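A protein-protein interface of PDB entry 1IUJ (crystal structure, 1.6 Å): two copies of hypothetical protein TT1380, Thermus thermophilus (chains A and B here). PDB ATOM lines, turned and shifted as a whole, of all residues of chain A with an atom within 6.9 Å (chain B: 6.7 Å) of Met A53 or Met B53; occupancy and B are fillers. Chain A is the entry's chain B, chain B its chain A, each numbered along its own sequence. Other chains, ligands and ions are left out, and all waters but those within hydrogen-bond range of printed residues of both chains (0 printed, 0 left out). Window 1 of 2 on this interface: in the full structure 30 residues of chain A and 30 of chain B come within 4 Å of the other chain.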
ATOM      1  N   VAL A   3     -13.858 -27.767   0.885  1.00  0.00           N
ATOM      2  CA  VAL A   3     -14.707 -26.923   0.051  1.00  0.00           C
ATOM      3  C   VAL A   3     -15.475 -25.939   0.911  1.00  0.00           C
ATOM      4  O   VAL A   3     -16.050 -26.326   1.957  1.00  0.00           O
ATOM      5  CB  VAL A   3     -15.728 -27.794  -0.751  1.00  0.00           C
ATOM      6  CG1 VAL A   3     -16.713 -26.948  -1.514  1.00  0.00           C
ATOM      7  CG2 VAL A   3     -15.005 -28.753  -1.669  1.00  0.00           C
ATOM      8  N   THR A   4     -15.526 -24.696   0.455  1.00  0.00           N
ATOM      9  CA  THR A   4     -16.435 -23.699   1.044  1.00  0.00           C
ATOM     10  C   THR A   4     -17.547 -23.356   0.073  1.00  0.00           C
ATOM     11  O   THR A   4     -17.339 -23.351  -1.144  1.00  0.00           O
ATOM     12  CB  THR A   4     -15.734 -22.400   1.458  1.00  0.00           C
ATOM     13  OG1 THR A   4     -15.087 -21.805   0.317  1.00  0.00           O
ATOM     14  CG2 THR A   4     -14.625 -22.656   2.441  1.00  0.00           C
ATOM     15  N   MET A   5     -18.730 -23.134   0.620  1.00  0.00           N
ATOM     16  CA  MET A   5     -19.849 -22.609  -0.157  1.00  0.00           C
ATOM     17  C   MET A   5     -20.366 -21.374   0.548  1.00  0.00           C
ATOM     18  O   MET A   5     -20.858 -21.446   1.668  1.00  0.00           O
ATOM     19  CB  MET A   5     -20.955 -23.656  -0.305  1.00  0.00           C
ATOM     20  CG  MET A   5     -20.508 -24.852  -1.073  1.00  0.00           C
ATOM     21  SD  MET A   5     -21.920 -25.886  -1.459  1.00  0.00           S
ATOM     22  CE  MET A   5     -21.041 -27.204  -2.117  1.00  0.00           C
ATOM     23  N   ASN A   6     -20.226 -20.220  -0.106  1.00  0.00           N
ATOM     24  CA  ASN A   6     -20.673 -18.968   0.481  1.00  0.00           C
ATOM     25  C   ASN A   6     -21.976 -18.641  -0.191  1.00  0.00           C
ATOM     26  O   ASN A   6     -21.992 -18.369  -1.408  1.00  0.00           O
ATOM     27  CB  ASN A   6     -19.639 -17.899   0.207  1.00  0.00           C
ATOM     28  CG  ASN A   6     -19.743 -16.697   1.158  1.00  0.00           C
ATOM     29  OD1 ASN A   6     -18.975 -15.726   1.011  1.00  0.00           O
ATOM     30  ND2 ASN A   6     -20.648 -16.745   2.115  1.00  0.00           N
ATOM     31  N   PHE A  22     -17.548 -10.088  -8.476  1.00  0.00           N
ATOM     32  CA  PHE A  22     -16.921 -11.355  -8.118  1.00  0.00           C
ATOM     33  C   PHE A  22     -15.924 -11.965  -9.120  1.00  0.00           C
ATOM     34  O   PHE A  22     -15.113 -12.846  -8.770  1.00  0.00           O
ATOM     35  CB  PHE A  22     -17.913 -12.422  -7.676  1.00  0.00           C
ATOM     36  CG  PHE A  22     -17.268 -13.427  -6.801  1.00  0.00           C
ATOM     37  CD1 PHE A  22     -17.514 -13.445  -5.432  1.00  0.00           C
ATOM     38  CD2 PHE A  22     -16.305 -14.300  -7.336  1.00  0.00           C
ATOM     39  CE1 PHE A  22     -16.855 -14.369  -4.634  1.00  0.00           C
ATOM     40  CE2 PHE A  22     -15.620 -15.222  -6.539  1.00  0.00           C
ATOM     41  CZ  PHE A  22     -15.905 -15.247  -5.186  1.00  0.00           C
ATOM     42  N   PHE A  35      -4.899 -23.298  -3.459  1.00  0.00           N
ATOM     43  CA  PHE A  35      -6.141 -23.044  -4.216  1.00  0.00           C
ATOM     44  C   PHE A  35      -6.239 -24.049  -5.362  1.00  0.00           C
ATOM     45  O   PHE A  35      -5.271 -24.254  -6.121  1.00  0.00           O
ATOM     46  CB  PHE A  35      -6.178 -21.606  -4.768  1.00  0.00           C
ATOM     47  CG  PHE A  35      -7.272 -21.361  -5.770  1.00  0.00           C
ATOM     48  CD1 PHE A  35      -8.572 -21.139  -5.341  1.00  0.00           C
ATOM     49  CD2 PHE A  35      -7.021 -21.358  -7.141  1.00  0.00           C
ATOM     50  CE1 PHE A  35      -9.634 -20.920  -6.256  1.00  0.00           C
ATOM     51  CE2 PHE A  35      -8.065 -21.127  -8.067  1.00  0.00           C
ATOM     52  CZ  PHE A  35      -9.373 -20.917  -7.631  1.00  0.00           C
ATOM     53  N   ARG A  37      -9.832 -24.546  -7.225  1.00  0.00           N
ATOM     54  CA  ARG A  37     -10.870 -24.143  -8.199  1.00  0.00           C
ATOM     55  C   ARG A  37     -11.905 -23.244  -7.555  1.00  0.00           C
ATOM     56  O   ARG A  37     -12.186 -23.407  -6.375  1.00  0.00           O
ATOM     57  CB  ARG A  37     -11.558 -25.367  -8.796  1.00  0.00           C
ATOM     58  CG  ARG A  37     -12.484 -25.120  -9.965  1.00  0.00           C
ATOM     59  CD  ARG A  37     -12.944 -26.401 -10.546  1.00  0.00           C
ATOM     60  NE  ARG A  37     -13.708 -26.203 -11.774  1.00  0.00           N
ATOM     61  CZ  ARG A  37     -14.242 -27.199 -12.448  1.00  0.00           C
ATOM     62  NH1 ARG A  37     -14.105 -28.449 -12.003  1.00  0.00           N
ATOM     63  NH2 ARG A  37     -14.943 -26.949 -13.546  1.00  0.00           N
ATOM     64  N   ASN A  38     -12.435 -22.275  -8.310  1.00  0.00           N
ATOM     65  CA  ASN A  38     -13.529 -21.424  -7.824  1.00  0.00           C
ATOM     66  C   ASN A  38     -14.661 -21.441  -8.838  1.00  0.00           C
ATOM     67  O   ASN A  38     -14.426 -21.302 -10.032  1.00  0.00           O
ATOM     68  CB  ASN A  38     -13.051 -19.973  -7.611  1.00  0.00           C
ATOM     69  CG  ASN A  38     -14.142 -19.054  -7.058  1.00  0.00           C
ATOM     70  OD1 ASN A  38     -14.702 -18.207  -7.785  1.00  0.00           O
ATOM     71  ND2 ASN A  38     -14.433 -19.188  -5.776  1.00  0.00           N
ATOM     72  N   LEU A  39     -15.897 -21.573  -8.373  1.00  0.00           N
ATOM     73  CA  LEU A  39     -17.057 -21.484  -9.268  1.00  0.00           C
ATOM     74  C   LEU A  39     -18.059 -20.527  -8.686  1.00  0.00           C
ATOM     75  O   LEU A  39     -18.272 -20.504  -7.468  1.00  0.00           O
ATOM     76  CB  LEU A  39     -17.694 -22.845  -9.498  1.00  0.00           C
ATOM     77  CG  LEU A  39     -16.776 -23.909 -10.092  1.00  0.00           C
ATOM     78  CD1 LEU A  39     -16.069 -24.743  -9.013  1.00  0.00           C
ATOM     79  CD2 LEU A  39     -17.568 -24.779 -11.033  1.00  0.00           C
ATOM     80  N   VAL A  40     -18.636 -19.676  -9.529  1.00  0.00           N
ATOM     81  CA  VAL A  40     -19.731 -18.855  -9.082  1.00  0.00           C
ATOM     82  C   VAL A  40     -20.995 -19.405  -9.733  1.00  0.00           C
ATOM     83  O   VAL A  40     -21.049 -19.618 -10.949  1.00  0.00           O
ATOM     84  CB  VAL A  40     -19.532 -17.377  -9.454  1.00  0.00           C
ATOM     85  CG1 VAL A  40     -20.698 -16.534  -8.894  1.00  0.00           C
ATOM     86  CG2 VAL A  40     -18.131 -16.854  -8.984  1.00  0.00           C
ATOM     87  N   LEU A  41     -21.984 -19.673  -8.898  1.00  0.00           N
ATOM     88  CA  LEU A  41     -23.171 -20.444  -9.295  1.00  0.00           C
ATOM     89  C   LEU A  41     -24.421 -19.594  -9.148  1.00  0.00           C
ATOM     90  O   LEU A  41     -24.771 -19.151  -8.060  1.00  0.00           O
ATOM     91  CB  LEU A  41     -23.264 -21.705  -8.413  1.00  0.00           C
ATOM     92  CG  LEU A  41     -22.101 -22.653  -8.432  1.00  0.00           C
ATOM     93  CD1 LEU A  41     -22.350 -23.793  -7.461  1.00  0.00           C
ATOM     94  CD2 LEU A  41     -21.818 -23.221  -9.828  1.00  0.00           C
ATOM     95  N   VAL A  51     -24.303 -19.148  -5.020  1.00  0.00           N
ATOM     96  CA  VAL A  51     -23.252 -19.864  -4.265  1.00  0.00           C
ATOM     97  C   VAL A  51     -21.887 -19.639  -4.860  1.00  0.00           C
ATOM     98  O   VAL A  51     -21.656 -19.898  -6.024  1.00  0.00           O
ATOM     99  CB  VAL A  51     -23.565 -21.388  -4.089  1.00  0.00           C
ATOM    100  CG1 VAL A  51     -22.396 -22.113  -3.438  1.00  0.00           C
ATOM    101  CG2 VAL A  51     -24.782 -21.552  -3.223  1.00  0.00           C
ATOM    102  N   VAL A  52     -20.947 -19.173  -4.034  1.00  0.00           N
ATOM    103  CA  VAL A  52     -19.558 -19.110  -4.467  1.00  0.00           C
ATOM    104  C   VAL A  52     -18.918 -20.348  -3.854  1.00  0.00           C
ATOM    105  O   VAL A  52     -18.828 -20.487  -2.608  1.00  0.00           O
ATOM    106  CB  VAL A  52     -18.851 -17.861  -3.979  1.00  0.00           C
ATOM    107  CG1 VAL A  52     -17.357 -17.958  -4.321  1.00  0.00           C
ATOM    108  CG2 VAL A  52     -19.517 -16.570  -4.510  1.00  0.00           C
ATOM    109  N   MET A  53     -18.453 -21.234  -4.723  1.00  0.00           N
ATOM    110  CA  MET A  53     -17.930 -22.516  -4.275  1.00  0.00           C
ATOM    111  C   MET A  53     -16.443 -22.538  -4.533  1.00  0.00           C
ATOM    112  O   MET A  53     -15.998 -22.299  -5.665  1.00  0.00           O
ATOM    113  CB  MET A  53     -18.569 -23.663  -5.048  1.00  0.00           C
ATOM    114  CG  MET A  53     -18.053 -24.989  -4.570  1.00  0.00           C
ATOM    115  SD  MET A  53     -18.950 -26.290  -5.349  1.00  0.00           S
ATOM    116  CE  MET A  53     -18.584 -26.019  -7.051  1.00  0.00           C
ATOM    117  N   THR A  54     -15.670 -22.847  -3.507  1.00  0.00           N
ATOM    118  CA  THR A  54     -14.223 -22.799  -3.660  1.00  0.00           C
ATOM    119  C   THR A  54     -13.613 -24.069  -3.143  1.00  0.00           C
ATOM    120  O   THR A  54     -14.008 -24.562  -2.073  1.00  0.00           O
ATOM    121  CB  THR A  54     -13.660 -21.599  -2.921  1.00  0.00           C
ATOM    122  OG1 THR A  54     -14.302 -20.400  -3.385  1.00  0.00           O
ATOM    123  CG2 THR A  54     -12.141 -21.411  -3.273  1.00  0.00           C
ATOM    124  N   LEU A  55     -12.734 -24.653  -3.955  1.00  0.00           N
ATOM    125  CA  LEU A  55     -12.070 -25.921  -3.651  1.00  0.00           C
ATOM    126  C   LEU A  55     -10.641 -25.640  -3.242  1.00  0.00           C
ATOM    127  O   LEU A  55      -9.931 -24.923  -3.949  1.00  0.00           O
ATOM    128  CB  LEU A  55     -12.055 -26.817  -4.899  1.00  0.00           C
ATOM    129  CG  LEU A  55     -13.310 -27.618  -5.241  1.00  0.00           C
ATOM    130  CD1 LEU A  55     -14.528 -26.709  -5.454  1.00  0.00           C
ATOM    131  CD2 LEU A  55     -12.977 -28.435  -6.513  1.00  0.00           C
ATOM    132  N   VAL B   3     -25.316 -27.314 -12.465  1.00  0.00           N
ATOM    133  CA  VAL B   3     -24.937 -27.970 -11.228  1.00  0.00           C
ATOM    134  C   VAL B   3     -26.174 -28.239 -10.393  1.00  0.00           C
ATOM    135  O   VAL B   3     -27.018 -27.356 -10.213  1.00  0.00           O
ATOM    136  CB  VAL B   3     -23.966 -27.074 -10.391  1.00  0.00           C
ATOM    137  CG1 VAL B   3     -23.720 -27.667  -8.996  1.00  0.00           C
ATOM    138  CG2 VAL B   3     -22.619 -26.846 -11.147  1.00  0.00           C
ATOM    139  N   THR B   4     -26.277 -29.460  -9.891  1.00  0.00           N
ATOM    140  CA  THR B   4     -27.256 -29.739  -8.841  1.00  0.00           C
ATOM    141  C   THR B   4     -26.552 -29.954  -7.501  1.00  0.00           C
ATOM    142  O   THR B   4     -25.458 -30.528  -7.419  1.00  0.00           O
ATOM    143  CB  THR B   4     -28.096 -31.010  -9.140  1.00  0.00           C
ATOM    144  OG1 THR B   4     -27.224 -32.132  -9.373  1.00  0.00           O
ATOM    145  CG2 THR B   4     -28.939 -30.851 -10.410  1.00  0.00           C
ATOM    146  N   MET B   5     -27.217 -29.530  -6.438  1.00  0.00           N
ATOM    147  CA  MET B   5     -26.751 -29.855  -5.074  1.00  0.00           C
ATOM    148  C   MET B   5     -27.922 -30.421  -4.312  1.00  0.00           C
ATOM    149  O   MET B   5     -28.919 -29.710  -4.126  1.00  0.00           O
ATOM    150  CB  MET B   5     -26.290 -28.584  -4.367  1.00  0.00           C
ATOM    151  CG  MET B   5     -25.265 -27.812  -5.096  1.00  0.00           C
ATOM    152  SD  MET B   5     -24.238 -26.848  -3.947  1.00  0.00           S
ATOM    153  CE  MET B   5     -23.275 -25.926  -5.091  1.00  0.00           C
ATOM    154  N   ASN B   6     -27.786 -31.663  -3.852  1.00  0.00           N
ATOM    155  CA  ASN B   6     -28.838 -32.283  -3.084  1.00  0.00           C
ATOM    156  C   ASN B   6     -28.350 -32.243  -1.642  1.00  0.00           C
ATOM    157  O   ASN B   6     -27.321 -32.872  -1.303  1.00  0.00           O
ATOM    158  CB  ASN B   6     -29.136 -33.729  -3.569  1.00  0.00           C
ATOM    159  CG  ASN B   6     -30.537 -34.222  -3.154  1.00  0.00           C
ATOM    160  OD1 ASN B   6     -30.834 -35.433  -3.242  1.00  0.00           O
ATOM    161  ND2 ASN B   6     -31.381 -33.313  -2.682  1.00  0.00           N
ATOM    162  N   PHE B  35     -22.936 -36.160 -18.248  1.00  0.00           N
ATOM    163  CA  PHE B  35     -22.363 -36.209 -16.875  1.00  0.00           C
ATOM    164  C   PHE B  35     -20.906 -35.755 -16.870  1.00  0.00           C
ATOM    165  O   PHE B  35     -20.105 -36.274 -17.669  1.00  0.00           O
ATOM    166  CB  PHE B  35     -22.410 -37.627 -16.301  1.00  0.00           C
ATOM    167  CG  PHE B  35     -21.657 -37.790 -14.995  1.00  0.00           C
ATOM    168  CD1 PHE B  35     -22.217 -37.350 -13.800  1.00  0.00           C
ATOM    169  CD2 PHE B  35     -20.401 -38.377 -14.966  1.00  0.00           C
ATOM    170  CE1 PHE B  35     -21.518 -37.497 -12.578  1.00  0.00           C
ATOM    171  CE2 PHE B  35     -19.710 -38.552 -13.744  1.00  0.00           C
ATOM    172  CZ  PHE B  35     -20.287 -38.109 -12.558  1.00  0.00           C
ATOM    173  N   ARG B  37     -19.114 -34.618 -13.415  1.00  0.00           N
ATOM    174  CA  ARG B  37     -18.469 -34.994 -12.175  1.00  0.00           C
ATOM    175  C   ARG B  37     -19.443 -34.991 -11.020  1.00  0.00           C
ATOM    176  O   ARG B  37     -20.422 -34.260 -11.036  1.00  0.00           O
ATOM    177  CB  ARG B  37     -17.353 -33.995 -11.939  1.00  0.00           C
ATOM    178  CG  ARG B  37     -16.452 -34.237 -10.729  1.00  0.00           C
ATOM    179  CD  ARG B  37     -15.493 -33.104 -10.611  1.00  0.00           C
ATOM    180  NE  ARG B  37     -14.439 -33.281  -9.609  1.00  0.00           N
ATOM    181  CZ  ARG B  37     -13.451 -32.406  -9.434  1.00  0.00           C
ATOM    182  NH1 ARG B  37     -13.378 -31.324 -10.194  1.00  0.00           N
ATOM    183  NH2 ARG B  37     -12.521 -32.597  -8.495  1.00  0.00           N
ATOM    184  N   ASN B  38     -19.157 -35.823 -10.026  1.00  0.00           N
ATOM    185  CA  ASN B  38     -19.979 -35.858  -8.817  1.00  0.00           C
ATOM    186  C   ASN B  38     -19.074 -35.813  -7.609  1.00  0.00           C
ATOM    187  O   ASN B  38     -18.012 -36.434  -7.605  1.00  0.00           O
ATOM    188  CB  ASN B  38     -20.773 -37.159  -8.821  1.00  0.00           C
ATOM    189  CG  ASN B  38     -21.589 -37.357  -7.576  1.00  0.00           C
ATOM    190  OD1 ASN B  38     -21.201 -38.149  -6.678  1.00  0.00           O
ATOM    191  ND2 ASN B  38     -22.748 -36.708  -7.523  1.00  0.00           N
ATOM    192  N   LEU B  39     -19.466 -35.038  -6.603  1.00  0.00           N
ATOM    193  CA  LEU B  39     -18.706 -34.943  -5.357  1.00  0.00           C
ATOM    194  C   LEU B  39     -19.674 -35.173  -4.221  1.00  0.00           C
ATOM    195  O   LEU B  39     -20.809 -34.696  -4.290  1.00  0.00           O
ATOM    196  CB  LEU B  39     -18.068 -33.569  -5.205  1.00  0.00           C
ATOM    197  CG  LEU B  39     -16.982 -33.478  -6.276  1.00  0.00           C
ATOM    198  CD1 LEU B  39     -17.393 -32.519  -7.347  1.00  0.00           C
ATOM    199  CD2 LEU B  39     -15.617 -33.166  -5.659  1.00  0.00           C
ATOM    200  N   VAL B  40     -19.268 -35.937  -3.214  1.00  0.00           N
ATOM    201  CA  VAL B  40     -20.068 -36.048  -1.993  1.00  0.00           C
ATOM    202  C   VAL B  40     -19.295 -35.256  -0.946  1.00  0.00           C
ATOM    203  O   VAL B  40     -18.121 -35.535  -0.742  1.00  0.00           O
ATOM    204  CB  VAL B  40     -20.250 -37.492  -1.526  1.00  0.00           C
ATOM    205  CG1 VAL B  40     -21.098 -37.556  -0.254  1.00  0.00           C
ATOM    206  CG2 VAL B  40     -20.900 -38.375  -2.645  1.00  0.00           C
ATOM    207  N   LEU B  41     -19.940 -34.260  -0.315  1.00  0.00           N
ATOM    208  CA  LEU B  41     -19.273 -33.337   0.636  1.00  0.00           C
ATOM    209  C   LEU B  41     -19.847 -33.547   2.050  1.00  0.00           C
ATOM    210  O   LEU B  41     -21.069 -33.461   2.278  1.00  0.00           O
ATOM    211  CB  LEU B  41     -19.566 -31.899   0.219  1.00  0.00           C
ATOM    212  CG  LEU B  41     -19.219 -31.590  -1.222  1.00  0.00           C
ATOM    213  CD1 LEU B  41     -19.686 -30.194  -1.584  1.00  0.00           C
ATOM    214  CD2 LEU B  41     -17.732 -31.772  -1.472  1.00  0.00           C
ATOM    215  N   VAL B  51     -23.792 -32.525   1.255  1.00  0.00           N
ATOM    216  CA  VAL B  51     -24.194 -32.066  -0.059  1.00  0.00           C
ATOM    217  C   VAL B  51     -23.693 -33.047  -1.115  1.00  0.00           C
ATOM    218  O   VAL B  51     -22.508 -33.353  -1.133  1.00  0.00           O
ATOM    219  CB  VAL B  51     -23.683 -30.673  -0.361  1.00  0.00           C
ATOM    220  CG1 VAL B  51     -23.935 -30.356  -1.824  1.00  0.00           C
ATOM    221  CG2 VAL B  51     -24.355 -29.637   0.556  1.00  0.00           C
ATOM    222  N   VAL B  52     -24.606 -33.550  -1.962  1.00  0.00           N
ATOM    223  CA  VAL B  52     -24.216 -34.319  -3.143  1.00  0.00           C
ATOM    224  C   VAL B  52     -24.256 -33.329  -4.324  1.00  0.00           C
ATOM    225  O   VAL B  52     -25.318 -32.820  -4.680  1.00  0.00           O
ATOM    226  CB  VAL B  52     -25.168 -35.530  -3.350  1.00  0.00           C
ATOM    227  CG1 VAL B  52     -24.850 -36.216  -4.680  1.00  0.00           C
ATOM    228  CG2 VAL B  52     -25.078 -36.474  -2.159  1.00  0.00           C
ATOM    229  N   MET B  53     -23.086 -33.063  -4.911  1.00  0.00           N
ATOM    230  CA  MET B  53     -22.938 -32.040  -5.945  1.00  0.00           C
ATOM    231  C   MET B  53     -22.620 -32.706  -7.266  1.00  0.00           C
ATOM    232  O   MET B  53     -21.682 -33.502  -7.350  1.00  0.00           O
ATOM    233  CB  MET B  53     -21.825 -31.039  -5.587  1.00  0.00           C
ATOM    234  CG  MET B  53     -21.717 -29.955  -6.623  1.00  0.00           C
ATOM    235  SD  MET B  53     -20.618 -28.732  -6.067  1.00  0.00           S
ATOM    236  CE  MET B  53     -19.092 -29.614  -6.158  1.00  0.00           C
ATOM    237  N   THR B  54     -23.403 -32.372  -8.290  1.00  0.00           N
ATOM    238  CA  THR B  54     -23.140 -32.948  -9.605  1.00  0.00           C
ATOM    239  C   THR B  54     -23.080 -31.879 -10.664  1.00  0.00           C
ATOM    240  O   THR B  54     -23.861 -30.913 -10.676  1.00  0.00           O
ATOM    241  CB  THR B  54     -24.212 -34.010  -9.977  1.00  0.00           C
ATOM    242  OG1 THR B  54     -24.389 -34.923  -8.891  1.00  0.00           O
ATOM    243  CG2 THR B  54     -23.686 -34.925 -11.094  1.00  0.00           C
ATOM    244  N   LEU B  55     -22.072 -32.031 -11.522  1.00  0.00           N
ATOM    245  CA  LEU B  55     -21.838 -31.158 -12.657  1.00  0.00           C
ATOM    246  C   LEU B  55     -22.287 -31.837 -13.941  1.00  0.00           C
ATOM    247  O   LEU B  55     -21.940 -32.998 -14.200  1.00  0.00           O
ATOM    248  CB  LEU B  55     -20.336 -30.842 -12.744  1.00  0.00           C
ATOM    249  CG  LEU B  55     -19.845 -29.825 -11.700  1.00  0.00           C
ATOM    250  CD1 LEU B  55     -20.004 -30.347 -10.277  1.00  0.00           C
ATOM    251  CD2 LEU B  55     -18.384 -29.482 -11.929  1.00  0.00           C
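The side-chain amide nitrogen (ND2) of Asn B38 sits close to the backbone carbonyl oxygen (O) of Met B53.
O of Arg A37 sits at hydrogen-bond distance from N of Leu A55, at 2.8 Å.
The backbone NH of Leu B55 lies within hydrogen-bond range of the backbone carbonyl oxygen of Arg B37.
N of Leu A41 is in hydrogen-bond range of O of Val A51 (2.9 Å).
The backbone carbonyl oxygen (O) of Val B51 sits at hydrogen-bond distance from the backbone NH (N) of Leu B41 (2.8 Å).
The backbone carbonyl oxygen of Met A53 is in hydrogen-bond range of the backbone NH of Leu A39.
Met A5 touches its own counterpart, Met B5.
Arg B37 touches its own counterpart, Arg A37.
Leu A41 touches Val B3, but with the chains exchanged Val A3 does not touch Leu B41 (4.1 Å).
Met A53 touches its own counterpart, Met B53.
Of chain B, only Met B53 (3.0 Å) comes within 4 Å of Met A53.
Of chain A, only Met A53 (3.0 Å) comes within 4 Å of Met B53.
Of the printed residues of chain A, Met B5 touches Met A5 and Leu A41.
Printed residues of chain B within 4 Å of Arg A37: Arg B37 (3.5 Å).
Of the printed residues of chain B, Leu A41 touches Val B3 and Met B5.
Of the printed residues of chain A, Arg B37 touches Arg A37.
Of the printed residues of chain B, Met A5 touches Met B5 (3.5 Å) and Leu B41 (3.3 Å).
Asn A6 touches none of the printed residues of chain B.
Asn B38 touches none of the printed residues of chain A.
Among the printed residues, pairs that only touch across the chains: Met A5 with Leu B41, Leu A41 with Val B3 and Leu A41 with Met B5.
NH1 of Arg B37 lies close to NH1 of Arg A37, 3.5 Å away.
The side-chain sulfur of Met A5 sits close to the side-chain sulfur of Met B5, at 3.5 Å.
SD of Met A53 sits close to SD of Met B53 (3.0 Å).
Hydrophobic or aromatic side chains of chain B that line the printed part of chain A: Val B3, Met B5, Leu B41 and Met B53.
Hydrophobic or aromatic side chains of chain A that line the printed part of chain B: Met A5, Leu A41 and Met A53.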
